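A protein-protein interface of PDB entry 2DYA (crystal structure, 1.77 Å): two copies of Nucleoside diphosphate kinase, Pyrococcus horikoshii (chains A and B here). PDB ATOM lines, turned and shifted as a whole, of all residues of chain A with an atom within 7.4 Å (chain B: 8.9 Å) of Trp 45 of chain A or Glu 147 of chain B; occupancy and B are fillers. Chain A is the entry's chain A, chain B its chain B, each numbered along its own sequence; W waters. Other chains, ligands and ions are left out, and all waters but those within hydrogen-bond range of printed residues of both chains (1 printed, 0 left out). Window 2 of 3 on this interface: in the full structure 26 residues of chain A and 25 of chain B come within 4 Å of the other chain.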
ATOM      1  N   PRO A  16     -15.345 -33.223 -16.995  1.00  0.00           N
ATOM      2  CA  PRO A  16     -14.609 -32.059 -17.496  1.00  0.00           C
ATOM      3  C   PRO A  16     -14.864 -31.702 -18.964  1.00  0.00           C
ATOM      4  O   PRO A  16     -14.969 -30.524 -19.301  1.00  0.00           O
ATOM      5  CB  PRO A  16     -13.152 -32.429 -17.218  1.00  0.00           C
ATOM      6  CG  PRO A  16     -13.265 -33.224 -15.956  1.00  0.00           C
ATOM      7  CD  PRO A  16     -14.437 -34.128 -16.266  1.00  0.00           C
ATOM      8  N   LYS A  42     -23.466 -29.616  -7.053  1.00  0.00           N
ATOM      9  CA  LYS A  42     -22.420 -28.626  -6.807  1.00  0.00           C
ATOM     10  C   LYS A  42     -21.221 -28.786  -7.728  1.00  0.00           C
ATOM     11  O   LYS A  42     -20.856 -29.899  -8.112  1.00  0.00           O
ATOM     12  CB  LYS A  42     -21.939 -28.714  -5.353  1.00  0.00           C
ATOM     13  CG  LYS A  42     -21.290 -30.046  -5.011  1.00  0.00           C
ATOM     14  CD  LYS A  42     -20.964 -30.141  -3.533  1.00  0.00           C
ATOM     15  CE  LYS A  42     -20.246 -31.440  -3.210  1.00  0.00           C
ATOM     16  NZ  LYS A  42     -19.830 -31.489  -1.783  1.00  0.00           N
ATOM     17  N   MET A  43     -20.617 -27.661  -8.090  1.00  0.00           N
ATOM     18  CA  MET A  43     -19.426 -27.688  -8.923  1.00  0.00           C
ATOM     19  C   MET A  43     -18.252 -27.844  -7.959  1.00  0.00           C
ATOM     20  O   MET A  43     -18.146 -27.122  -6.962  1.00  0.00           O
ATOM     21  CB  MET A  43     -19.276 -26.391  -9.723  1.00  0.00           C
ATOM     22  CG  MET A  43     -17.955 -26.302 -10.490  1.00  0.00           C
ATOM     23  SD  MET A  43     -17.815 -24.858 -11.580  1.00  0.00           S
ATOM     24  CE  MET A  43     -18.561 -25.510 -13.101  1.00  0.00           C
ATOM     25  N   ILE A  44     -17.394 -28.814  -8.237  1.00  0.00           N
ATOM     26  CA  ILE A  44     -16.232 -29.064  -7.399  1.00  0.00           C
ATOM     27  C   ILE A  44     -15.070 -29.403  -8.313  1.00  0.00           C
ATOM     28  O   ILE A  44     -15.260 -29.611  -9.510  1.00  0.00           O
ATOM     29  CB  ILE A  44     -16.460 -30.271  -6.444  1.00  0.00           C
ATOM     30  CG1 ILE A  44     -16.739 -31.540  -7.263  1.00  0.00           C
ATOM     31  CG2 ILE A  44     -17.615 -29.975  -5.479  1.00  0.00           C
ATOM     32  CD1 ILE A  44     -16.895 -32.808  -6.429  1.00  0.00           C
ATOM     33  N   TRP A  45     -13.865 -29.428  -7.760  1.00  0.00           N
ATOM     34  CA  TRP A  45     -12.693 -29.799  -8.539  1.00  0.00           C
ATOM     35  C   TRP A  45     -12.094 -30.998  -7.812  1.00  0.00           C
ATOM     36  O   TRP A  45     -11.443 -30.861  -6.777  1.00  0.00           O
ATOM     37  CB  TRP A  45     -11.676 -28.661  -8.619  1.00  0.00           C
ATOM     38  CG  TRP A  45     -10.723 -28.829  -9.775  1.00  0.00           C
ATOM     39  CD1 TRP A  45     -10.239 -30.010 -10.272  1.00  0.00           C
ATOM     40  CD2 TRP A  45     -10.123 -27.789 -10.561  1.00  0.00           C
ATOM     41  NE1 TRP A  45      -9.379 -29.768 -11.316  1.00  0.00           N
ATOM     42  CE2 TRP A  45      -9.289 -28.416 -11.516  1.00  0.00           C
ATOM     43  CE3 TRP A  45     -10.208 -26.390 -10.554  1.00  0.00           C
ATOM     44  CZ2 TRP A  45      -8.548 -27.690 -12.456  1.00  0.00           C
ATOM     45  CZ3 TRP A  45      -9.471 -25.669 -11.488  1.00  0.00           C
ATOM     46  CH2 TRP A  45      -8.651 -26.323 -12.428  1.00  0.00           C
ATOM     47  N   ILE A  46     -12.343 -32.180  -8.361  1.00  0.00           N
ATOM     48  CA  ILE A  46     -11.877 -33.430  -7.775  1.00  0.00           C
ATOM     49  C   ILE A  46     -10.370 -33.586  -7.857  1.00  0.00           C
ATOM     50  O   ILE A  46      -9.768 -33.317  -8.894  1.00  0.00           O
ATOM     51  CB  ILE A  46     -12.534 -34.642  -8.484  1.00  0.00           C
ATOM     52  CG1 ILE A  46     -14.063 -34.519  -8.423  1.00  0.00           C
ATOM     53  CG2 ILE A  46     -12.076 -35.940  -7.833  1.00  0.00           C
ATOM     54  CD1 ILE A  46     -14.802 -35.552  -9.256  1.00  0.00           C
ATOM     55  N   ASP A  47      -9.762 -34.019  -6.758  1.00  0.00           N
ATOM     56  CA  ASP A  47      -8.320 -34.238  -6.742  1.00  0.00           C
ATOM     57  C   ASP A  47      -8.066 -35.728  -6.944  1.00  0.00           C
ATOM     58  O   ASP A  47      -8.991 -36.539  -6.849  1.00  0.00           O
ATOM     59  CB  ASP A  47      -7.700 -33.744  -5.425  1.00  0.00           C
ATOM     60  CG  ASP A  47      -8.258 -34.450  -4.198  1.00  0.00           C
ATOM     61  OD1 ASP A  47      -7.834 -34.089  -3.078  1.00  0.00           O
ATOM     62  OD2 ASP A  47      -9.105 -35.357  -4.338  1.00  0.00           O
ATOM     63  N   ARG A  48      -6.821 -36.090  -7.226  1.00  0.00           N
ATOM     64  CA  ARG A  48      -6.478 -37.487  -7.465  1.00  0.00           C
ATOM     65  C   ARG A  48      -6.945 -38.463  -6.386  1.00  0.00           C
ATOM     66  O   ARG A  48      -7.460 -39.530  -6.707  1.00  0.00           O
ATOM     67  CB  ARG A  48      -4.969 -37.628  -7.673  1.00  0.00           C
ATOM     68  CG  ARG A  48      -4.429 -36.793  -8.818  1.00  0.00           C
ATOM     69  CD  ARG A  48      -3.038 -37.251  -9.237  1.00  0.00           C
ATOM     70  NE  ARG A  48      -3.060 -38.452 -10.076  1.00  0.00           N
ATOM     71  CZ  ARG A  48      -3.459 -38.473 -11.347  1.00  0.00           C
ATOM     72  NH1 ARG A  48      -3.874 -37.357 -11.930  1.00  0.00           N
ATOM     73  NH2 ARG A  48      -3.431 -39.607 -12.038  1.00  0.00           N
ATOM     74  N   LEU A  50      -9.518 -38.313  -4.180  1.00  0.00           N
ATOM     75  CA  LEU A  50     -10.963 -38.528  -4.230  1.00  0.00           C
ATOM     76  C   LEU A  50     -11.357 -39.264  -5.507  1.00  0.00           C
ATOM     77  O   LEU A  50     -12.226 -40.137  -5.487  1.00  0.00           O
ATOM     78  CB  LEU A  50     -11.708 -37.184  -4.152  1.00  0.00           C
ATOM     79  CG  LEU A  50     -13.243 -37.190  -4.232  1.00  0.00           C
ATOM     80  CD1 LEU A  50     -13.828 -38.039  -3.103  1.00  0.00           C
ATOM     81  CD2 LEU A  50     -13.767 -35.761  -4.152  1.00  0.00           C
ATOM     82  N   ASP A  69      -6.579 -38.639 -14.577  1.00  0.00           N
ATOM     83  CA  ASP A  69      -6.141 -37.356 -15.130  1.00  0.00           C
ATOM     84  C   ASP A  69      -7.343 -36.653 -15.757  1.00  0.00           C
ATOM     85  O   ASP A  69      -7.520 -35.444 -15.617  1.00  0.00           O
ATOM     86  CB  ASP A  69      -5.083 -37.541 -16.225  1.00  0.00           C
ATOM     87  CG  ASP A  69      -3.843 -38.249 -15.736  1.00  0.00           C
ATOM     88  OD1 ASP A  69      -3.385 -37.963 -14.611  1.00  0.00           O
ATOM     89  OD2 ASP A  69      -3.312 -39.087 -16.494  1.00  0.00           O
ATOM     90  N   ILE A  71     -10.812 -37.120 -15.197  1.00  0.00           N
ATOM     91  CA  ILE A  71     -11.841 -36.672 -14.268  1.00  0.00           C
ATOM     92  C   ILE A  71     -11.384 -35.503 -13.391  1.00  0.00           C
ATOM     93  O   ILE A  71     -12.208 -34.780 -12.832  1.00  0.00           O
ATOM     94  CB  ILE A  71     -12.325 -37.852 -13.370  1.00  0.00           C
ATOM     95  CG1 ILE A  71     -13.655 -37.493 -12.695  1.00  0.00           C
ATOM     96  CG2 ILE A  71     -11.264 -38.200 -12.326  1.00  0.00           C
ATOM     97  CD1 ILE A  71     -14.856 -37.551 -13.631  1.00  0.00           C
ATOM     98  N   THR A  72     -10.074 -35.312 -13.273  1.00  0.00           N
ATOM     99  CA  THR A  72      -9.543 -34.221 -12.456  1.00  0.00           C
ATOM    100  C   THR A  72      -8.999 -33.075 -13.307  1.00  0.00           C
ATOM    101  O   THR A  72      -8.395 -32.137 -12.782  1.00  0.00           O
ATOM    102  CB  THR A  72      -8.398 -34.709 -11.543  1.00  0.00           C
ATOM    103  OG1 THR A  72      -7.325 -35.206 -12.354  1.00  0.00           O
ATOM    104  CG2 THR A  72      -8.882 -35.809 -10.607  1.00  0.00           C
ATOM    105  N   LYS A  73      -9.226 -33.142 -14.615  1.00  0.00           N
ATOM    106  CA  LYS A  73      -8.721 -32.127 -15.536  1.00  0.00           C
ATOM    107  C   LYS A  73      -9.238 -30.709 -15.265  1.00  0.00           C
ATOM    108  O   LYS A  73      -8.465 -29.753 -15.264  1.00  0.00           O
ATOM    109  CB  LYS A  73      -9.028 -32.549 -16.975  1.00  0.00           C
ATOM    110  CG  LYS A  73      -8.262 -31.780 -18.039  1.00  0.00           C
ATOM    111  CD  LYS A  73      -8.509 -32.391 -19.414  1.00  0.00           C
ATOM    112  CE  LYS A  73      -7.810 -31.618 -20.523  1.00  0.00           C
ATOM    113  NZ  LYS A  73      -6.330 -31.705 -20.414  1.00  0.00           N
ATOM    114  N   THR A  74     -10.544 -30.569 -15.056  1.00  0.00           N
ATOM    115  CA  THR A  74     -11.143 -29.266 -14.764  1.00  0.00           C
ATOM    116  C   THR A  74     -12.249 -29.536 -13.756  1.00  0.00           C
ATOM    117  O   THR A  74     -12.495 -30.688 -13.399  1.00  0.00           O
ATOM    118  CB  THR A  74     -11.796 -28.602 -16.020  1.00  0.00           C
ATOM    119  OG1 THR A  74     -12.971 -29.331 -16.398  1.00  0.00           O
ATOM    120  CG2 THR A  74     -10.826 -28.571 -17.193  1.00  0.00           C
ATOM    121  N   PRO A  75     -12.917 -28.482 -13.267  1.00  0.00           N
ATOM    122  CA  PRO A  75     -13.991 -28.746 -12.305  1.00  0.00           C
ATOM    123  C   PRO A  75     -15.099 -29.563 -12.971  1.00  0.00           C
ATOM    124  O   PRO A  75     -15.193 -29.618 -14.198  1.00  0.00           O
ATOM    125  CB  PRO A  75     -14.460 -27.348 -11.918  1.00  0.00           C
ATOM    126  CG  PRO A  75     -13.205 -26.547 -12.018  1.00  0.00           C
ATOM    127  CD  PRO A  75     -12.600 -27.044 -13.311  1.00  0.00           C
ATOM    128  N   VAL A  76     -15.924 -30.204 -12.155  1.00  0.00           N
ATOM    129  CA  VAL A  76     -17.035 -31.007 -12.656  1.00  0.00           C
ATOM    130  C   VAL A  76     -18.275 -30.618 -11.859  1.00  0.00           C
ATOM    131  O   VAL A  76     -18.201 -29.816 -10.930  1.00  0.00           O
ATOM    132  CB  VAL A  76     -16.781 -32.530 -12.449  1.00  0.00           C
ATOM    133  CG1 VAL A  76     -15.605 -32.989 -13.291  1.00  0.00           C
ATOM    134  CG2 VAL A  76     -16.521 -32.823 -10.968  1.00  0.00           C
ATOM    135  N   VAL A  77     -19.423 -31.161 -12.245  1.00  0.00           N
ATOM    136  CA  VAL A  77     -20.652 -30.906 -11.510  1.00  0.00           C
ATOM    137  C   VAL A  77     -21.142 -32.272 -11.033  1.00  0.00           C
ATOM    138  O   VAL A  77     -21.453 -33.146 -11.848  1.00  0.00           O
ATOM    139  CB  VAL A  77     -21.748 -30.247 -12.393  1.00  0.00           C
ATOM    140  CG1 VAL A  77     -23.003 -29.989 -11.558  1.00  0.00           C
ATOM    141  CG2 VAL A  77     -21.241 -28.949 -12.978  1.00  0.00           C
ATOM    142  N   ARG B   9     -17.637 -10.857 -12.286  1.00  0.00           N
ATOM    143  CA  ARG B   9     -18.337 -12.021 -11.767  1.00  0.00           C
ATOM    144  C   ARG B   9     -19.640 -11.541 -11.141  1.00  0.00           C
ATOM    145  O   ARG B   9     -19.656 -10.564 -10.390  1.00  0.00           O
ATOM    146  CB  ARG B   9     -17.501 -12.737 -10.703  1.00  0.00           C
ATOM    147  CG  ARG B   9     -16.347 -13.573 -11.231  1.00  0.00           C
ATOM    148  CD  ARG B   9     -15.640 -14.278 -10.079  1.00  0.00           C
ATOM    149  NE  ARG B   9     -14.560 -15.149 -10.532  1.00  0.00           N
ATOM    150  CZ  ARG B   9     -13.815 -15.894  -9.721  1.00  0.00           C
ATOM    151  NH1 ARG B   9     -14.031 -15.874  -8.411  1.00  0.00           N
ATOM    152  NH2 ARG B   9     -12.855 -16.664 -10.216  1.00  0.00           N
ATOM    153  N   LYS B  37     -18.849 -18.079 -18.193  1.00  0.00           N
ATOM    154  CA  LYS B  37     -18.229 -19.214 -17.514  1.00  0.00           C
ATOM    155  C   LYS B  37     -18.765 -19.414 -16.104  1.00  0.00           C
ATOM    156  O   LYS B  37     -18.834 -18.468 -15.321  1.00  0.00           O
ATOM    157  CB  LYS B  37     -16.708 -19.026 -17.441  1.00  0.00           C
ATOM    158  CG  LYS B  37     -15.970 -20.203 -16.785  1.00  0.00           C
ATOM    159  CD  LYS B  37     -14.468 -19.954 -16.697  1.00  0.00           C
ATOM    160  CE  LYS B  37     -13.837 -19.836 -18.074  1.00  0.00           C
ATOM    161  NZ  LYS B  37     -12.401 -19.426 -18.000  1.00  0.00           N
ATOM    162  N   ILE B  38     -19.137 -20.650 -15.786  1.00  0.00           N
ATOM    163  CA  ILE B  38     -19.642 -20.989 -14.459  1.00  0.00           C
ATOM    164  C   ILE B  38     -18.432 -21.320 -13.577  1.00  0.00           C
ATOM    165  O   ILE B  38     -17.843 -22.395 -13.705  1.00  0.00           O
ATOM    166  CB  ILE B  38     -20.575 -22.222 -14.511  1.00  0.00           C
ATOM    167  CG1 ILE B  38     -21.749 -21.947 -15.449  1.00  0.00           C
ATOM    168  CG2 ILE B  38     -21.081 -22.554 -13.118  1.00  0.00           C
ATOM    169  CD1 ILE B  38     -22.629 -23.155 -15.705  1.00  0.00           C
ATOM    170  N   VAL B  39     -18.056 -20.399 -12.694  1.00  0.00           N
ATOM    171  CA  VAL B  39     -16.906 -20.627 -11.822  1.00  0.00           C
ATOM    172  C   VAL B  39     -17.300 -21.187 -10.453  1.00  0.00           C
ATOM    173  O   VAL B  39     -16.452 -21.668  -9.695  1.00  0.00           O
ATOM    174  CB  VAL B  39     -16.079 -19.328 -11.636  1.00  0.00           C
ATOM    175  CG1 VAL B  39     -15.531 -18.871 -12.987  1.00  0.00           C
ATOM    176  CG2 VAL B  39     -16.932 -18.245 -10.998  1.00  0.00           C
ATOM    177  N   GLY B  40     -18.594 -21.132 -10.150  1.00  0.00           N
ATOM    178  CA  GLY B  40     -19.098 -21.646  -8.890  1.00  0.00           C
ATOM    179  C   GLY B  40     -20.567 -21.996  -9.037  1.00  0.00           C
ATOM    180  O   GLY B  40     -21.284 -21.332  -9.789  1.00  0.00           O
ATOM    181  N   GLU B  82     -18.893 -15.788 -14.721  1.00  0.00           N
ATOM    182  CA  GLU B  82     -17.762 -14.934 -15.036  1.00  0.00           C
ATOM    183  C   GLU B  82     -17.681 -14.651 -16.534  1.00  0.00           C
ATOM    184  O   GLU B  82     -17.865 -15.549 -17.358  1.00  0.00           O
ATOM    185  CB  GLU B  82     -16.477 -15.598 -14.562  1.00  0.00           C
ATOM    186  CG  GLU B  82     -15.259 -14.716 -14.657  1.00  0.00           C
ATOM    187  CD  GLU B  82     -14.042 -15.382 -14.067  1.00  0.00           C
ATOM    188  OE1 GLU B  82     -13.562 -16.376 -14.653  1.00  0.00           O
ATOM    189  OE2 GLU B  82     -13.576 -14.918 -13.008  1.00  0.00           O
ATOM    190  N   PRO B 142     -14.167 -18.790  -1.090  1.00  0.00           N
ATOM    191  CA  PRO B 142     -13.168 -18.767  -2.165  1.00  0.00           C
ATOM    192  C   PRO B 142     -12.852 -20.162  -2.714  1.00  0.00           C
ATOM    193  O   PRO B 142     -12.590 -20.330  -3.908  1.00  0.00           O
ATOM    194  CB  PRO B 142     -11.959 -18.117  -1.490  1.00  0.00           C
ATOM    195  CG  PRO B 142     -12.601 -17.169  -0.514  1.00  0.00           C
ATOM    196  CD  PRO B 142     -13.699 -18.025   0.082  1.00  0.00           C
ATOM    197  N   GLU B 143     -12.893 -21.154  -1.827  1.00  0.00           N
ATOM    198  CA  GLU B 143     -12.604 -22.544  -2.170  1.00  0.00           C
ATOM    199  C   GLU B 143     -13.657 -23.205  -3.067  1.00  0.00           C
ATOM    200  O   GLU B 143     -13.445 -24.313  -3.568  1.00  0.00           O
ATOM    201  CB  GLU B 143     -12.449 -23.371  -0.888  1.00  0.00           C
ATOM    202  CG  GLU B 143     -11.272 -22.973   0.006  1.00  0.00           C
ATOM    203  CD  GLU B 143     -11.414 -21.583   0.615  1.00  0.00           C
ATOM    204  OE1 GLU B 143     -12.520 -21.245   1.090  1.00  0.00           O
ATOM    205  OE2 GLU B 143     -10.411 -20.833   0.633  1.00  0.00           O
ATOM    206  N   GLU B 144     -14.785 -22.528  -3.260  1.00  0.00           N
ATOM    207  CA  GLU B 144     -15.872 -23.045  -4.090  1.00  0.00           C
ATOM    208  C   GLU B 144     -15.914 -22.371  -5.457  1.00  0.00           C
ATOM    209  O   GLU B 144     -16.782 -22.665  -6.275  1.00  0.00           O
ATOM    210  CB  GLU B 144     -17.212 -22.828  -3.396  1.00  0.00           C
ATOM    211  CG  GLU B 144     -17.359 -23.543  -2.066  1.00  0.00           C
ATOM    212  CD  GLU B 144     -18.668 -23.206  -1.379  1.00  0.00           C
ATOM    213  OE1 GLU B 144     -18.847 -22.039  -0.976  1.00  0.00           O
ATOM    214  OE2 GLU B 144     -19.523 -24.104  -1.245  1.00  0.00           O
ATOM    215  N   LEU B 145     -14.986 -21.456  -5.697  1.00  0.00           N
ATOM    216  CA  LEU B 145     -14.928 -20.745  -6.964  1.00  0.00           C
ATOM    217  C   LEU B 145     -13.667 -21.210  -7.670  1.00  0.00           C
ATOM    218  O   LEU B 145     -12.602 -21.292  -7.057  1.00  0.00           O
ATOM    219  CB  LEU B 145     -14.904 -19.236  -6.716  1.00  0.00           C
ATOM    220  CG  LEU B 145     -16.143 -18.718  -5.979  1.00  0.00           C
ATOM    221  CD1 LEU B 145     -15.976 -17.250  -5.630  1.00  0.00           C
ATOM    222  CD2 LEU B 145     -17.374 -18.927  -6.850  1.00  0.00           C
ATOM    223  N   PHE B 146     -13.783 -21.510  -8.959  1.00  0.00           N
ATOM    224  CA  PHE B 146     -12.651 -22.039  -9.705  1.00  0.00           C
ATOM    225  C   PHE B 146     -12.181 -21.255 -10.917  1.00  0.00           C
ATOM    226  O   PHE B 146     -12.927 -20.492 -11.531  1.00  0.00           O
ATOM    227  CB  PHE B 146     -12.971 -23.477 -10.130  1.00  0.00           C
ATOM    228  CG  PHE B 146     -13.496 -24.327  -9.011  1.00  0.00           C
ATOM    229  CD1 PHE B 146     -12.645 -24.791  -8.012  1.00  0.00           C
ATOM    230  CD2 PHE B 146     -14.857 -24.609  -8.919  1.00  0.00           C
ATOM    231  CE1 PHE B 146     -13.144 -25.520  -6.932  1.00  0.00           C
ATOM    232  CE2 PHE B 146     -15.367 -25.335  -7.842  1.00  0.00           C
ATOM    233  CZ  PHE B 146     -14.510 -25.791  -6.846  1.00  0.00           C
ATOM    234  N   GLU B 147     -10.918 -21.478 -11.253  1.00  0.00           N
ATOM    235  CA  GLU B 147     -10.283 -20.848 -12.394  1.00  0.00           C
ATOM    236  C   GLU B 147      -9.928 -21.983 -13.339  1.00  0.00           C
ATOM    237  O   GLU B 147      -9.109 -22.839 -13.012  1.00  0.00           O
ATOM    238  CB  GLU B 147      -9.016 -20.123 -11.954  1.00  0.00           C
ATOM    239  CG  GLU B 147      -8.346 -19.330 -13.055  1.00  0.00           C
ATOM    240  CD  GLU B 147      -7.161 -18.541 -12.541  1.00  0.00           C
ATOM    241  OE1 GLU B 147      -6.147 -19.167 -12.159  1.00  0.00           O
ATOM    242  OE2 GLU B 147      -7.252 -17.293 -12.509  1.00  0.00           O
ATOM    243  N   TYR B 148     -10.564 -22.000 -14.503  1.00  0.00           N
ATOM    244  CA  TYR B 148     -10.310 -23.051 -15.475  1.00  0.00           C
ATOM    245  C   TYR B 148     -10.722 -22.561 -16.850  1.00  0.00           C
ATOM    246  O   TYR B 148     -11.548 -21.660 -16.978  1.00  0.00           O
ATOM    247  CB  TYR B 148     -11.105 -24.305 -15.113  1.00  0.00           C
ATOM    248  CG  TYR B 148     -12.597 -24.149 -15.281  1.00  0.00           C
ATOM    249  CD1 TYR B 148     -13.217 -24.431 -16.504  1.00  0.00           C
ATOM    250  CD2 TYR B 148     -13.391 -23.705 -14.225  1.00  0.00           C
ATOM    251  CE1 TYR B 148     -14.596 -24.273 -16.668  1.00  0.00           C
ATOM    252  CE2 TYR B 148     -14.765 -23.545 -14.376  1.00  0.00           C
ATOM    253  CZ  TYR B 148     -15.363 -23.831 -15.598  1.00  0.00           C
ATOM    254  OH  TYR B 148     -16.727 -23.688 -15.738  1.00  0.00           O
ATOM    255  N   PRO B 149     -10.148 -23.152 -17.898  1.00  0.00           N
ATOM    256  CA  PRO B 149     -10.491 -22.728 -19.252  1.00  0.00           C
ATOM    257  C   PRO B 149     -11.722 -23.388 -19.863  1.00  0.00           C
ATOM    258  O   PRO B 149     -11.933 -24.591 -19.730  1.00  0.00           O
ATOM    259  CB  PRO B 149      -9.224 -23.054 -20.034  1.00  0.00           C
ATOM    260  CG  PRO B 149      -8.763 -24.313 -19.375  1.00  0.00           C
ATOM    261  CD  PRO B 149      -8.946 -24.006 -17.900  1.00  0.00           C
ATOM    262  N   ARG B 150     -12.542 -22.578 -20.519  1.00  0.00           N
ATOM    263  CA  ARG B 150     -13.705 -23.091 -21.213  1.00  0.00           C
ATOM    264  C   ARG B 150     -13.170 -23.380 -22.618  1.00  0.00           C
ATOM    265  O   ARG B 150     -12.115 -22.867 -23.002  1.00  0.00           O
ATOM    266  CB  ARG B 150     -14.828 -22.047 -21.239  1.00  0.00           C
ATOM    267  CG  ARG B 150     -15.900 -22.271 -20.166  1.00  0.00           C
ATOM    268  CD  ARG B 150     -16.853 -23.388 -20.571  1.00  0.00           C
ATOM    269  NE  ARG B 150     -17.732 -22.957 -21.658  1.00  0.00           N
ATOM    270  CZ  ARG B 150     -18.848 -22.252 -21.487  1.00  0.00           C
ATOM    271  NH1 ARG B 150     -19.240 -21.905 -20.268  1.00  0.00           N
ATOM    272  NH2 ARG B 150     -19.561 -21.869 -22.540  1.00  0.00           N
ATOM    273  N   ASP B 153     -11.918 -20.355 -24.898  1.00  0.00           N
ATOM    274  CA  ASP B 153     -11.122 -19.306 -24.255  1.00  0.00           C
ATOM    275  C   ASP B 153      -9.896 -18.881 -25.064  1.00  0.00           C
ATOM    276  O   ASP B 153      -9.610 -17.690 -25.185  1.00  0.00           O
ATOM    277  CB  ASP B 153     -10.673 -19.741 -22.853  1.00  0.00           C
ATOM    278  CG  ASP B 153     -11.811 -19.741 -21.842  1.00  0.00           C
ATOM    279  OD1 ASP B 153     -12.965 -19.486 -22.231  1.00  0.00           O
ATOM    280  OD2 ASP B 153     -11.549 -20.001 -20.649  1.00  0.00           O
HETATM  281  O   HOH W   1     -19.066 -24.337  -6.731  1.00  0.00           O
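The backbone carbonyl oxygen (O) of Ile 38 of chain B lies close to the side-chain sulfur (SD) of Met 43 of chain A (3.3 Å).
The backbone carbonyl oxygen of Thr 72 of chain A is in hydrogen-bond range of the indole nitrogen of Trp 45 of chain A (3.0 Å). O of Ile 44 of chain A is in hydrogen-bond range of N of Val 76 of chain A. The backbone carbonyl oxygen (O) of Ile 38 of chain B is in hydrogen-bond range of the side-chain hydroxyl (OH) of Tyr 148 of chain B, 2.7 Å away. O of Val 39 of chain B lies within hydrogen-bond range of N of Phe 146 of chain B, at 2.8 Å. NZ of Lys 37 of chain B is in hydrogen-bond range of O of Tyr 148 of chain B, 2.6 Å away.
Met 43 of chain A touches Val 39 of chain B (SD to C, 3.9 Å). Met 43 of chain A touches Phe 146 of chain B. Met 43 of chain A touches Tyr 148 of chain B. Ile 44 of chain A touches Phe 146 of chain B. N of Trp 45 of chain A touches CZ of Phe 146 of chain B (3.8 Å). Trp 45 of chain A touches Glu 147 of chain B (CZ3 to O, 3.2 Å). Phe 146 of chain B touches Pro 75 of chain A. CD of Pro 75 of chain A touches CG of Tyr 148 of chain B, 3.5 Å away.
Printed residues of chain B within 4 Å of Met 43 of chain A: Ile 38, Val 39, Phe 146 and Tyr 148. Of chain B, only Phe 146 (3.7 Å) comes within 4 Å of Ile 44 of chain A. Of chain B, only Phe 146 (3.8 Å) and Glu 147 (3.2 Å) come within 4 Å of Trp 45 of chain A. Of the printed residues of chain B, Pro 75 of chain A touches Phe 146 (3.6 Å) and Tyr 148 (3.5 Å). Of the printed residues of chain A, Val 39 of chain B touches Met 43 (3.9 Å). Printed residues of chain A within 4 Å of Phe 146 of chain B: Met 43, Ile 44, Trp 45 and Pro 75. Glu 147 of chain B touches just one residue of chain A: Trp 45 (3.2 Å). The nearest printed residue of chain A that does not touch Val 39 of chain B is Pro 75 of chain A (6.3 Å).
Of the 17 printed residues of chain A, 4 touch a printed residue of chain B. Hydrophobic or aromatic side chains of chain A that line the printed part of chain B: Met 43, Trp 45 and Pro 75. Among the printed residues, no Asp or Glu carboxylate lies within 4 Å of a Lys or Arg side-chain nitrogen of the other chain.
No position is printed for both chains. Of the 9 pairs that touch across the chains among the printed residues, none has its exchanged pair printed and touching as well.
Water W1 bridges the backbone carbonyl oxygen of Glu 144 of chain B and the backbone carbonyl oxygen of Met 43 of chain A.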
